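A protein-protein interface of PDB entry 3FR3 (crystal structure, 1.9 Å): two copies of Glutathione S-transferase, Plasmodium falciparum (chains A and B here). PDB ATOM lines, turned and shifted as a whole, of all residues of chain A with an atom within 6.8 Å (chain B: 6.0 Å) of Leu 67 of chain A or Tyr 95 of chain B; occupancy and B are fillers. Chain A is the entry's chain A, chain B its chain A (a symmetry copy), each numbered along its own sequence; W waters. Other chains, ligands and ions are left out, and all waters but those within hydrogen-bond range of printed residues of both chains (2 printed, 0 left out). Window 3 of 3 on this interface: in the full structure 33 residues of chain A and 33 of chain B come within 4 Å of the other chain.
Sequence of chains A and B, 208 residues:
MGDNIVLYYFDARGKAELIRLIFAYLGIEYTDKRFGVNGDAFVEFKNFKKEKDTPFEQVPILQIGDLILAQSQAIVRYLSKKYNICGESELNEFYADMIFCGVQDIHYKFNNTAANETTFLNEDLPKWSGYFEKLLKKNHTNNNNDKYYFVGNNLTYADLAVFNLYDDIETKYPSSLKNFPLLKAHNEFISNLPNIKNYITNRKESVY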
ATOM      1  N   ILE A  61      -7.315   3.537  17.490  1.00  0.00           N
ATOM      2  CA  ILE A  61      -8.760   3.473  17.682  1.00  0.00           C
ATOM      3  C   ILE A  61      -8.977   3.291  19.176  1.00  0.00           C
ATOM      4  O   ILE A  61      -8.284   2.500  19.797  1.00  0.00           O
ATOM      5  CB  ILE A  61      -9.415   2.223  16.977  1.00  0.00           C
ATOM      6  CG1 ILE A  61      -9.381   2.387  15.450  1.00  0.00           C
ATOM      7  CG2 ILE A  61     -10.819   1.976  17.576  1.00  0.00           C
ATOM      8  CD1 ILE A  61     -10.250   3.514  14.935  1.00  0.00           C
ATOM      9  N   LEU A  62      -9.922   4.038  19.746  1.00  0.00           N
ATOM     10  CA  LEU A  62     -10.321   3.865  21.116  1.00  0.00           C
ATOM     11  C   LEU A  62     -11.755   3.435  21.118  1.00  0.00           C
ATOM     12  O   LEU A  62     -12.604   4.144  20.638  1.00  0.00           O
ATOM     13  CB  LEU A  62     -10.202   5.176  21.908  1.00  0.00           C
ATOM     14  CG  LEU A  62     -10.588   5.061  23.384  1.00  0.00           C
ATOM     15  CD1 LEU A  62      -9.568   4.212  24.126  1.00  0.00           C
ATOM     16  CD2 LEU A  62     -10.673   6.448  24.003  1.00  0.00           C
ATOM     17  N   GLN A  63     -11.973   2.254  21.692  1.00  0.00           N
ATOM     18  CA  GLN A  63     -13.273   1.668  21.840  1.00  0.00           C
ATOM     19  C   GLN A  63     -13.688   1.767  23.293  1.00  0.00           C
ATOM     20  O   GLN A  63     -12.962   1.334  24.182  1.00  0.00           O
ATOM     21  CB  GLN A  63     -13.274   0.219  21.379  1.00  0.00           C
ATOM     22  CG  GLN A  63     -14.750  -0.294  21.208  1.00  0.00           C
ATOM     23  CD  GLN A  63     -14.792  -1.680  20.684  1.00  0.00           C
ATOM     24  OE1 GLN A  63     -15.726  -2.429  20.993  1.00  0.00           O
ATOM     25  NE2 GLN A  63     -13.791  -2.055  19.896  1.00  0.00           N
ATOM     26  N   ILE A  64     -14.826   2.395  23.526  1.00  0.00           N
ATOM     27  CA  ILE A  64     -15.342   2.565  24.872  1.00  0.00           C
ATOM     28  C   ILE A  64     -16.708   1.889  24.760  1.00  0.00           C
ATOM     29  O   ILE A  64     -17.609   2.380  24.061  1.00  0.00           O
ATOM     30  CB  ILE A  64     -15.525   4.052  25.258  1.00  0.00           C
ATOM     31  CG1 ILE A  64     -14.177   4.827  25.110  1.00  0.00           C
ATOM     32  CG2 ILE A  64     -16.133   4.156  26.693  1.00  0.00           C
ATOM     33  CD1 ILE A  64     -14.347   6.373  25.214  1.00  0.00           C
ATOM     34  N   GLY A  65     -16.799   0.717  25.372  1.00  0.00           N
ATOM     35  CA  GLY A  65     -17.975  -0.136  25.204  1.00  0.00           C
ATOM     36  C   GLY A  65     -18.133  -0.505  23.750  1.00  0.00           C
ATOM     37  O   GLY A  65     -17.254  -1.139  23.162  1.00  0.00           O
ATOM     38  N   ASP A  66     -19.239  -0.088  23.158  1.00  0.00           N
ATOM     39  CA  ASP A  66     -19.478  -0.337  21.741  1.00  0.00           C
ATOM     40  C   ASP A  66     -19.075   0.852  20.843  1.00  0.00           C
ATOM     41  O   ASP A  66     -19.060   0.715  19.619  1.00  0.00           O
ATOM     42  CB  ASP A  66     -20.958  -0.633  21.497  1.00  0.00           C
ATOM     43  CG  ASP A  66     -21.335  -2.071  21.842  1.00  0.00           C
ATOM     44  OD1 ASP A  66     -22.473  -2.247  22.275  1.00  0.00           O
ATOM     45  OD2 ASP A  66     -20.509  -3.008  21.660  1.00  0.00           O
ATOM     46  N   LEU A  67     -18.769   1.995  21.456  1.00  0.00           N
ATOM     47  CA  LEU A  67     -18.423   3.223  20.733  1.00  0.00           C
ATOM     48  C   LEU A  67     -16.973   3.193  20.226  1.00  0.00           C
ATOM     49  O   LEU A  67     -16.039   3.073  21.016  1.00  0.00           O
ATOM     50  CB  LEU A  67     -18.613   4.401  21.693  1.00  0.00           C
ATOM     51  CG  LEU A  67     -18.448   5.845  21.214  1.00  0.00           C
ATOM     52  CD1 LEU A  67     -19.384   6.187  20.097  1.00  0.00           C
ATOM     53  CD2 LEU A  67     -18.614   6.832  22.381  1.00  0.00           C
ATOM     54  N   ILE A  68     -16.811   3.298  18.915  1.00  0.00           N
ATOM     55  CA  ILE A  68     -15.501   3.303  18.227  1.00  0.00           C
ATOM     56  C   ILE A  68     -15.104   4.778  17.919  1.00  0.00           C
ATOM     57  O   ILE A  68     -15.832   5.485  17.178  1.00  0.00           O
ATOM     58  CB  ILE A  68     -15.620   2.516  16.921  1.00  0.00           C
ATOM     59  CG1 ILE A  68     -15.809   1.006  17.233  1.00  0.00           C
ATOM     60  CG2 ILE A  68     -14.378   2.699  15.969  1.00  0.00           C
ATOM     61  CD1 ILE A  68     -15.600   0.125  16.041  1.00  0.00           C
ATOM     62  N   LEU A  69     -13.992   5.229  18.497  1.00  0.00           N
ATOM     63  CA  LEU A  69     -13.454   6.584  18.249  1.00  0.00           C
ATOM     64  C   LEU A  69     -12.113   6.466  17.495  1.00  0.00           C
ATOM     65  O   LEU A  69     -11.264   5.647  17.838  1.00  0.00           O
ATOM     66  CB  LEU A  69     -13.227   7.347  19.595  1.00  0.00           C
ATOM     67  CG  LEU A  69     -14.381   7.292  20.641  1.00  0.00           C
ATOM     68  CD1 LEU A  69     -14.022   8.116  21.814  1.00  0.00           C
ATOM     69  CD2 LEU A  69     -15.657   7.805  20.070  1.00  0.00           C
ATOM     70  N   ALA A  70     -11.938   7.277  16.453  1.00  0.00           N
ATOM     71  CA  ALA A  70     -10.703   7.289  15.698  1.00  0.00           C
ATOM     72  C   ALA A  70     -10.119   8.703  15.746  1.00  0.00           C
ATOM     73  O   ALA A  70     -10.784   9.667  16.169  1.00  0.00           O
ATOM     74  CB  ALA A  70     -10.962   6.889  14.228  1.00  0.00           C
ATOM     75  N   ALA A  74      -8.411  14.031  17.897  1.00  0.00           N
ATOM     76  CA  ALA A  74      -9.801  14.140  18.293  1.00  0.00           C
ATOM     77  C   ALA A  74     -10.087  13.341  19.568  1.00  0.00           C
ATOM     78  O   ALA A  74     -10.897  13.785  20.400  1.00  0.00           O
ATOM     79  CB  ALA A  74     -10.722  13.628  17.085  1.00  0.00           C
ATOM     80  N   TYR A  78     -11.361  14.998  23.095  1.00  0.00           N
ATOM     81  CA  TYR A  78     -12.595  14.479  23.703  1.00  0.00           C
ATOM     82  C   TYR A  78     -12.358  14.065  25.149  1.00  0.00           C
ATOM     83  O   TYR A  78     -13.119  14.403  26.074  1.00  0.00           O
ATOM     84  CB  TYR A  78     -13.004  13.236  22.856  1.00  0.00           C
ATOM     85  CG  TYR A  78     -14.126  12.421  23.472  1.00  0.00           C
ATOM     86  CD1 TYR A  78     -13.862  11.187  24.108  1.00  0.00           C
ATOM     87  CD2 TYR A  78     -15.447  12.866  23.405  1.00  0.00           C
ATOM     88  CE1 TYR A  78     -14.920  10.439  24.684  1.00  0.00           C
ATOM     89  CE2 TYR A  78     -16.497  12.116  23.969  1.00  0.00           C
ATOM     90  CZ  TYR A  78     -16.212  10.919  24.608  1.00  0.00           C
ATOM     91  OH  TYR A  78     -17.248  10.171  25.160  1.00  0.00           O
ATOM     92  N   GLU B  90     -21.952  16.100  22.847  1.00  0.00           N
ATOM     93  CA  GLU B  90     -20.537  15.709  23.085  1.00  0.00           C
ATOM     94  C   GLU B  90     -20.048  14.703  22.027  1.00  0.00           C
ATOM     95  O   GLU B  90     -18.928  14.824  21.538  1.00  0.00           O
ATOM     96  CB  GLU B  90     -20.414  15.175  24.495  1.00  0.00           C
ATOM     97  CG  GLU B  90     -19.554  13.995  24.738  1.00  0.00           C
ATOM     98  CD  GLU B  90     -19.886  13.370  26.116  1.00  0.00           C
ATOM     99  OE1 GLU B  90     -19.891  12.118  26.199  1.00  0.00           O
ATOM    100  OE2 GLU B  90     -20.165  14.144  27.080  1.00  0.00           O
ATOM    101  N   LEU B  91     -20.899  13.740  21.647  1.00  0.00           N
ATOM    102  CA  LEU B  91     -20.520  12.789  20.570  1.00  0.00           C
ATOM    103  C   LEU B  91     -20.451  13.418  19.174  1.00  0.00           C
ATOM    104  O   LEU B  91     -19.512  13.169  18.411  1.00  0.00           O
ATOM    105  CB  LEU B  91     -21.465  11.566  20.557  1.00  0.00           C
ATOM    106  CG  LEU B  91     -21.029  10.358  19.717  1.00  0.00           C
ATOM    107  CD1 LEU B  91     -19.683   9.850  20.197  1.00  0.00           C
ATOM    108  CD2 LEU B  91     -22.102   9.250  19.749  1.00  0.00           C
ATOM    109  N   ASN B  92     -21.412  14.263  18.839  1.00  0.00           N
ATOM    110  CA  ASN B  92     -21.328  14.970  17.551  1.00  0.00           C
ATOM    111  C   ASN B  92     -20.150  15.939  17.420  1.00  0.00           C
ATOM    112  O   ASN B  92     -19.615  16.119  16.310  1.00  0.00           O
ATOM    113  CB  ASN B  92     -22.646  15.670  17.169  1.00  0.00           C
ATOM    114  CG  ASN B  92     -23.717  14.671  16.688  1.00  0.00           C
ATOM    115  OD1 ASN B  92     -24.896  15.014  16.555  1.00  0.00           O
ATOM    116  ND2 ASN B  92     -23.306  13.428  16.451  1.00  0.00           N
ATOM    117  N   GLU B  93     -19.776  16.585  18.528  1.00  0.00           N
ATOM    118  CA  GLU B  93     -18.597  17.443  18.557  1.00  0.00           C
ATOM    119  C   GLU B  93     -17.369  16.561  18.273  1.00  0.00           C
ATOM    120  O   GLU B  93     -16.507  16.935  17.472  1.00  0.00           O
ATOM    121  CB  GLU B  93     -18.504  18.159  19.939  1.00  0.00           C
ATOM    122  CG  GLU B  93     -17.281  19.043  20.083  1.00  0.00           C
ATOM    123  CD  GLU B  93     -17.168  19.703  21.505  1.00  0.00           C
ATOM    124  OE1 GLU B  93     -16.269  20.545  21.701  1.00  0.00           O
ATOM    125  OE2 GLU B  93     -17.929  19.327  22.440  1.00  0.00           O
ATOM    126  N   PHE B  94     -17.301  15.403  18.932  1.00  0.00           N
ATOM    127  CA  PHE B  94     -16.200  14.469  18.689  1.00  0.00           C
ATOM    128  C   PHE B  94     -16.214  14.069  17.224  1.00  0.00           C
ATOM    129  O   PHE B  94     -15.157  14.050  16.601  1.00  0.00           O
ATOM    130  CB  PHE B  94     -16.287  13.169  19.532  1.00  0.00           C
ATOM    131  CG  PHE B  94     -15.383  12.097  19.001  1.00  0.00           C
ATOM    132  CD1 PHE B  94     -13.997  12.190  19.218  1.00  0.00           C
ATOM    133  CD2 PHE B  94     -15.844  11.157  18.080  1.00  0.00           C
ATOM    134  CE1 PHE B  94     -13.101  11.251  18.615  1.00  0.00           C
ATOM    135  CE2 PHE B  94     -14.958  10.236  17.526  1.00  0.00           C
ATOM    136  CZ  PHE B  94     -13.624  10.279  17.782  1.00  0.00           C
ATOM    137  N   TYR B  95     -17.370  13.654  16.696  1.00  0.00           N
ATOM    138  CA  TYR B  95     -17.425  13.263  15.290  1.00  0.00           C
ATOM    139  C   TYR B  95     -17.015  14.374  14.302  1.00  0.00           C
ATOM    140  O   TYR B  95     -16.345  14.093  13.304  1.00  0.00           O
ATOM    141  CB  TYR B  95     -18.808  12.717  14.866  1.00  0.00           C
ATOM    142  CG  TYR B  95     -19.097  11.361  15.465  1.00  0.00           C
ATOM    143  CD1 TYR B  95     -18.137  10.329  15.422  1.00  0.00           C
ATOM    144  CD2 TYR B  95     -20.328  11.091  16.040  1.00  0.00           C
ATOM    145  CE1 TYR B  95     -18.412   9.078  15.942  1.00  0.00           C
ATOM    146  CE2 TYR B  95     -20.605   9.850  16.558  1.00  0.00           C
ATOM    147  CZ  TYR B  95     -19.674   8.864  16.519  1.00  0.00           C
ATOM    148  OH  TYR B  95     -19.992   7.644  17.085  1.00  0.00           O
ATOM    149  N   ALA B  96     -17.426  15.618  14.546  1.00  0.00           N
ATOM    150  CA  ALA B  96     -16.994  16.687  13.651  1.00  0.00           C
ATOM    151  C   ALA B  96     -15.474  16.815  13.647  1.00  0.00           C
ATOM    152  O   ALA B  96     -14.850  17.045  12.614  1.00  0.00           O
ATOM    153  CB  ALA B  96     -17.627  17.998  14.050  1.00  0.00           C
ATOM    154  N   ASP B  97     -14.902  16.701  14.840  1.00  0.00           N
ATOM    155  CA  ASP B  97     -13.441  16.817  15.020  1.00  0.00           C
ATOM    156  C   ASP B  97     -12.785  15.627  14.311  1.00  0.00           C
ATOM    157  O   ASP B  97     -11.806  15.792  13.555  1.00  0.00           O
ATOM    158  CB  ASP B  97     -13.182  16.686  16.521  1.00  0.00           C
ATOM    159  CG  ASP B  97     -11.789  17.106  16.936  1.00  0.00           C
ATOM    160  OD1 ASP B  97     -11.581  17.235  18.166  1.00  0.00           O
ATOM    161  OD2 ASP B  97     -10.894  17.210  16.067  1.00  0.00           O
ATOM    162  N   MET B  98     -13.306  14.422  14.548  1.00  0.00           N
ATOM    163  CA  MET B  98     -12.722  13.213  13.890  1.00  0.00           C
ATOM    164  C   MET B  98     -12.724  13.389  12.380  1.00  0.00           C
ATOM    165  O   MET B  98     -11.753  13.075  11.672  1.00  0.00           O
ATOM    166  CB  MET B  98     -13.523  11.943  14.277  1.00  0.00           C
ATOM    167  CG  MET B  98     -12.923  10.612  13.702  1.00  0.00           C
ATOM    168  SD  MET B  98     -14.198   9.368  13.974  1.00  0.00           S
ATOM    169  CE  MET B  98     -15.299   9.689  12.584  1.00  0.00           C
ATOM    170  N   ILE B  99     -13.859  13.852  11.855  1.00  0.00           N
ATOM    171  CA  ILE B  99     -13.955  14.029  10.368  1.00  0.00           C
ATOM    172  C   ILE B  99     -12.977  15.120   9.856  1.00  0.00           C
ATOM    173  O   ILE B  99     -12.257  14.933   8.856  1.00  0.00           O
ATOM    174  CB  ILE B  99     -15.438  14.338   9.945  1.00  0.00           C
ATOM    175  CG1 ILE B  99     -16.324  13.106  10.222  1.00  0.00           C
ATOM    176  CG2 ILE B  99     -15.495  14.800   8.490  1.00  0.00           C
ATOM    177  CD1 ILE B  99     -17.802  13.437  10.205  1.00  0.00           C
ATOM    178  N   PHE B 100     -12.894  16.239  10.586  1.00  0.00           N
ATOM    179  CA  PHE B 100     -11.877  17.260  10.219  1.00  0.00           C
ATOM    180  C   PHE B 100     -10.467  16.683  10.239  1.00  0.00           C
ATOM    181  O   PHE B 100      -9.664  16.942   9.347  1.00  0.00           O
ATOM    182  CB  PHE B 100     -12.020  18.476  11.157  1.00  0.00           C
ATOM    183  CG  PHE B 100     -11.098  19.589  10.848  1.00  0.00           C
ATOM    184  CD1 PHE B 100     -10.916  20.016   9.541  1.00  0.00           C
ATOM    185  CD2 PHE B 100     -10.432  20.251  11.873  1.00  0.00           C
ATOM    186  CE1 PHE B 100     -10.048  21.071   9.248  1.00  0.00           C
ATOM    187  CE2 PHE B 100      -9.566  21.330  11.593  1.00  0.00           C
ATOM    188  CZ  PHE B 100      -9.372  21.730  10.297  1.00  0.00           C
ATOM    189  N   VAL B 151     -22.611  15.535  10.288  1.00  0.00           N
ATOM    190  CA  VAL B 151     -22.767  15.363  11.708  1.00  0.00           C
ATOM    191  C   VAL B 151     -24.093  15.994  12.109  1.00  0.00           C
ATOM    192  O   VAL B 151     -24.334  17.185  11.848  1.00  0.00           O
ATOM    193  CB  VAL B 151     -21.606  16.124  12.462  1.00  0.00           C
ATOM    194  CG1 VAL B 151     -21.851  16.067  13.943  1.00  0.00           C
ATOM    195  CG2 VAL B 151     -20.252  15.502  12.127  1.00  0.00           C
ATOM    196  N   ALA B 158     -17.039  20.586   9.866  1.00  0.00           N
ATOM    197  CA  ALA B 158     -16.595  19.356   9.164  1.00  0.00           C
ATOM    198  C   ALA B 158     -17.201  19.395   7.723  1.00  0.00           C
ATOM    199  O   ALA B 158     -16.526  19.026   6.740  1.00  0.00           O
ATOM    200  CB  ALA B 158     -17.037  18.112   9.915  1.00  0.00           C
HETATM  201  O   HOH W   1     -18.201   5.552  16.329  1.00  0.00           O
HETATM  202  O   HOH W   2     -12.919  15.525  19.910  1.00  0.00           O
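CD1 of Leu 67 of chain A touches CD1 of Leu 91 of chain B, 3.7 Å away. CD1 of Leu 67 of chain A touches OH of Tyr 95 of chain B, at 3.4 Å. CB of Leu 69 of chain A touches CZ of Phe 94 of chain B, 3.5 Å away. Ala 70 of chain A touches Phe 94 of chain B (O to CZ, 3.3 Å). Ala 70 of chain A touches Met 98 of chain B. Phe 94 of chain B touches Ala 74 of chain A (CD1 to O, 3.7 Å). Ala 74 of chain A touches Asp 97 of chain B. N of Met 98 of chain B touches CB of Ala 74 of chain A, 3.7 Å away. CD1 of Phe 94 of chain B touches CB of Tyr 78 of chain A (3.9 Å).
The side-chain carboxylate of Glu 90 of chain B is in hydrogen-bond range of the side-chain hydroxyl of Tyr 78 of chain A, at 3.4 Å.
Leu 67 of chain A touches two residues of chain B. Tyr 95 of chain B touches just one residue of chain A: Leu 67. Of the printed residues of chain A, Met 98 of chain B touches Ala 70 and Ala 74. Of the printed residues of chain B, Ala 70 of chain A touches Phe 94 (3.3 Å) and Met 98 (3.4 Å). Ala 96 of chain B touches none of the printed residues of chain A. The nearest printed residue of chain B that does not touch Leu 67 of chain A is Phe 94 of chain B (6.4 Å). The nearest residue of chain A that does not touch Tyr 95 of chain B is Ile 68 of chain A (4.6 Å). The nearest printed residue of chain A that does not touch Glu 90 of chain B is Leu 67 of chain A (6.6 Å).
Water W1 bridges the backbone carbonyl oxygen (O) of Ile 68 of chain A (2.5 Å) and the side-chain hydroxyl (OH) of Tyr 95 of chain B (2.9 Å). Water W2 lies within hydrogen-bond range of the backbone carbonyl oxygen (O) of Ala 74 of chain A (2.7 Å) and the side-chain carboxylate (OD1) of Asp 97 of chain B (2.8 Å).
No position is printed for both chains. Of the 10 pairs that touch across the chains among the printed residues, none has its exchanged pair printed and touching as well.
The backbone carbonyl oxygen (O) of Leu 62 of chain A lies within hydrogen-bond range of the backbone NH (N) of Leu 69 of chain A.
Of the 13 printed residues of chain B, 6 touch a printed residue of chain A. Printed residues of chain B that touch a printed residue of chain A: Glu 90, Leu 91, Phe 94, Tyr 95, Asp 97 and Met 98. Hydrophobic or aromatic side chains of chain B within 4 Å of the printed part of chain A: Leu 91, Phe 94, Tyr 95 and Met 98. Along chain B the printed residues that touch a printed residue of chain A span positions 90 to 98. Among the printed residues, 10 pairs touch across the chains.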
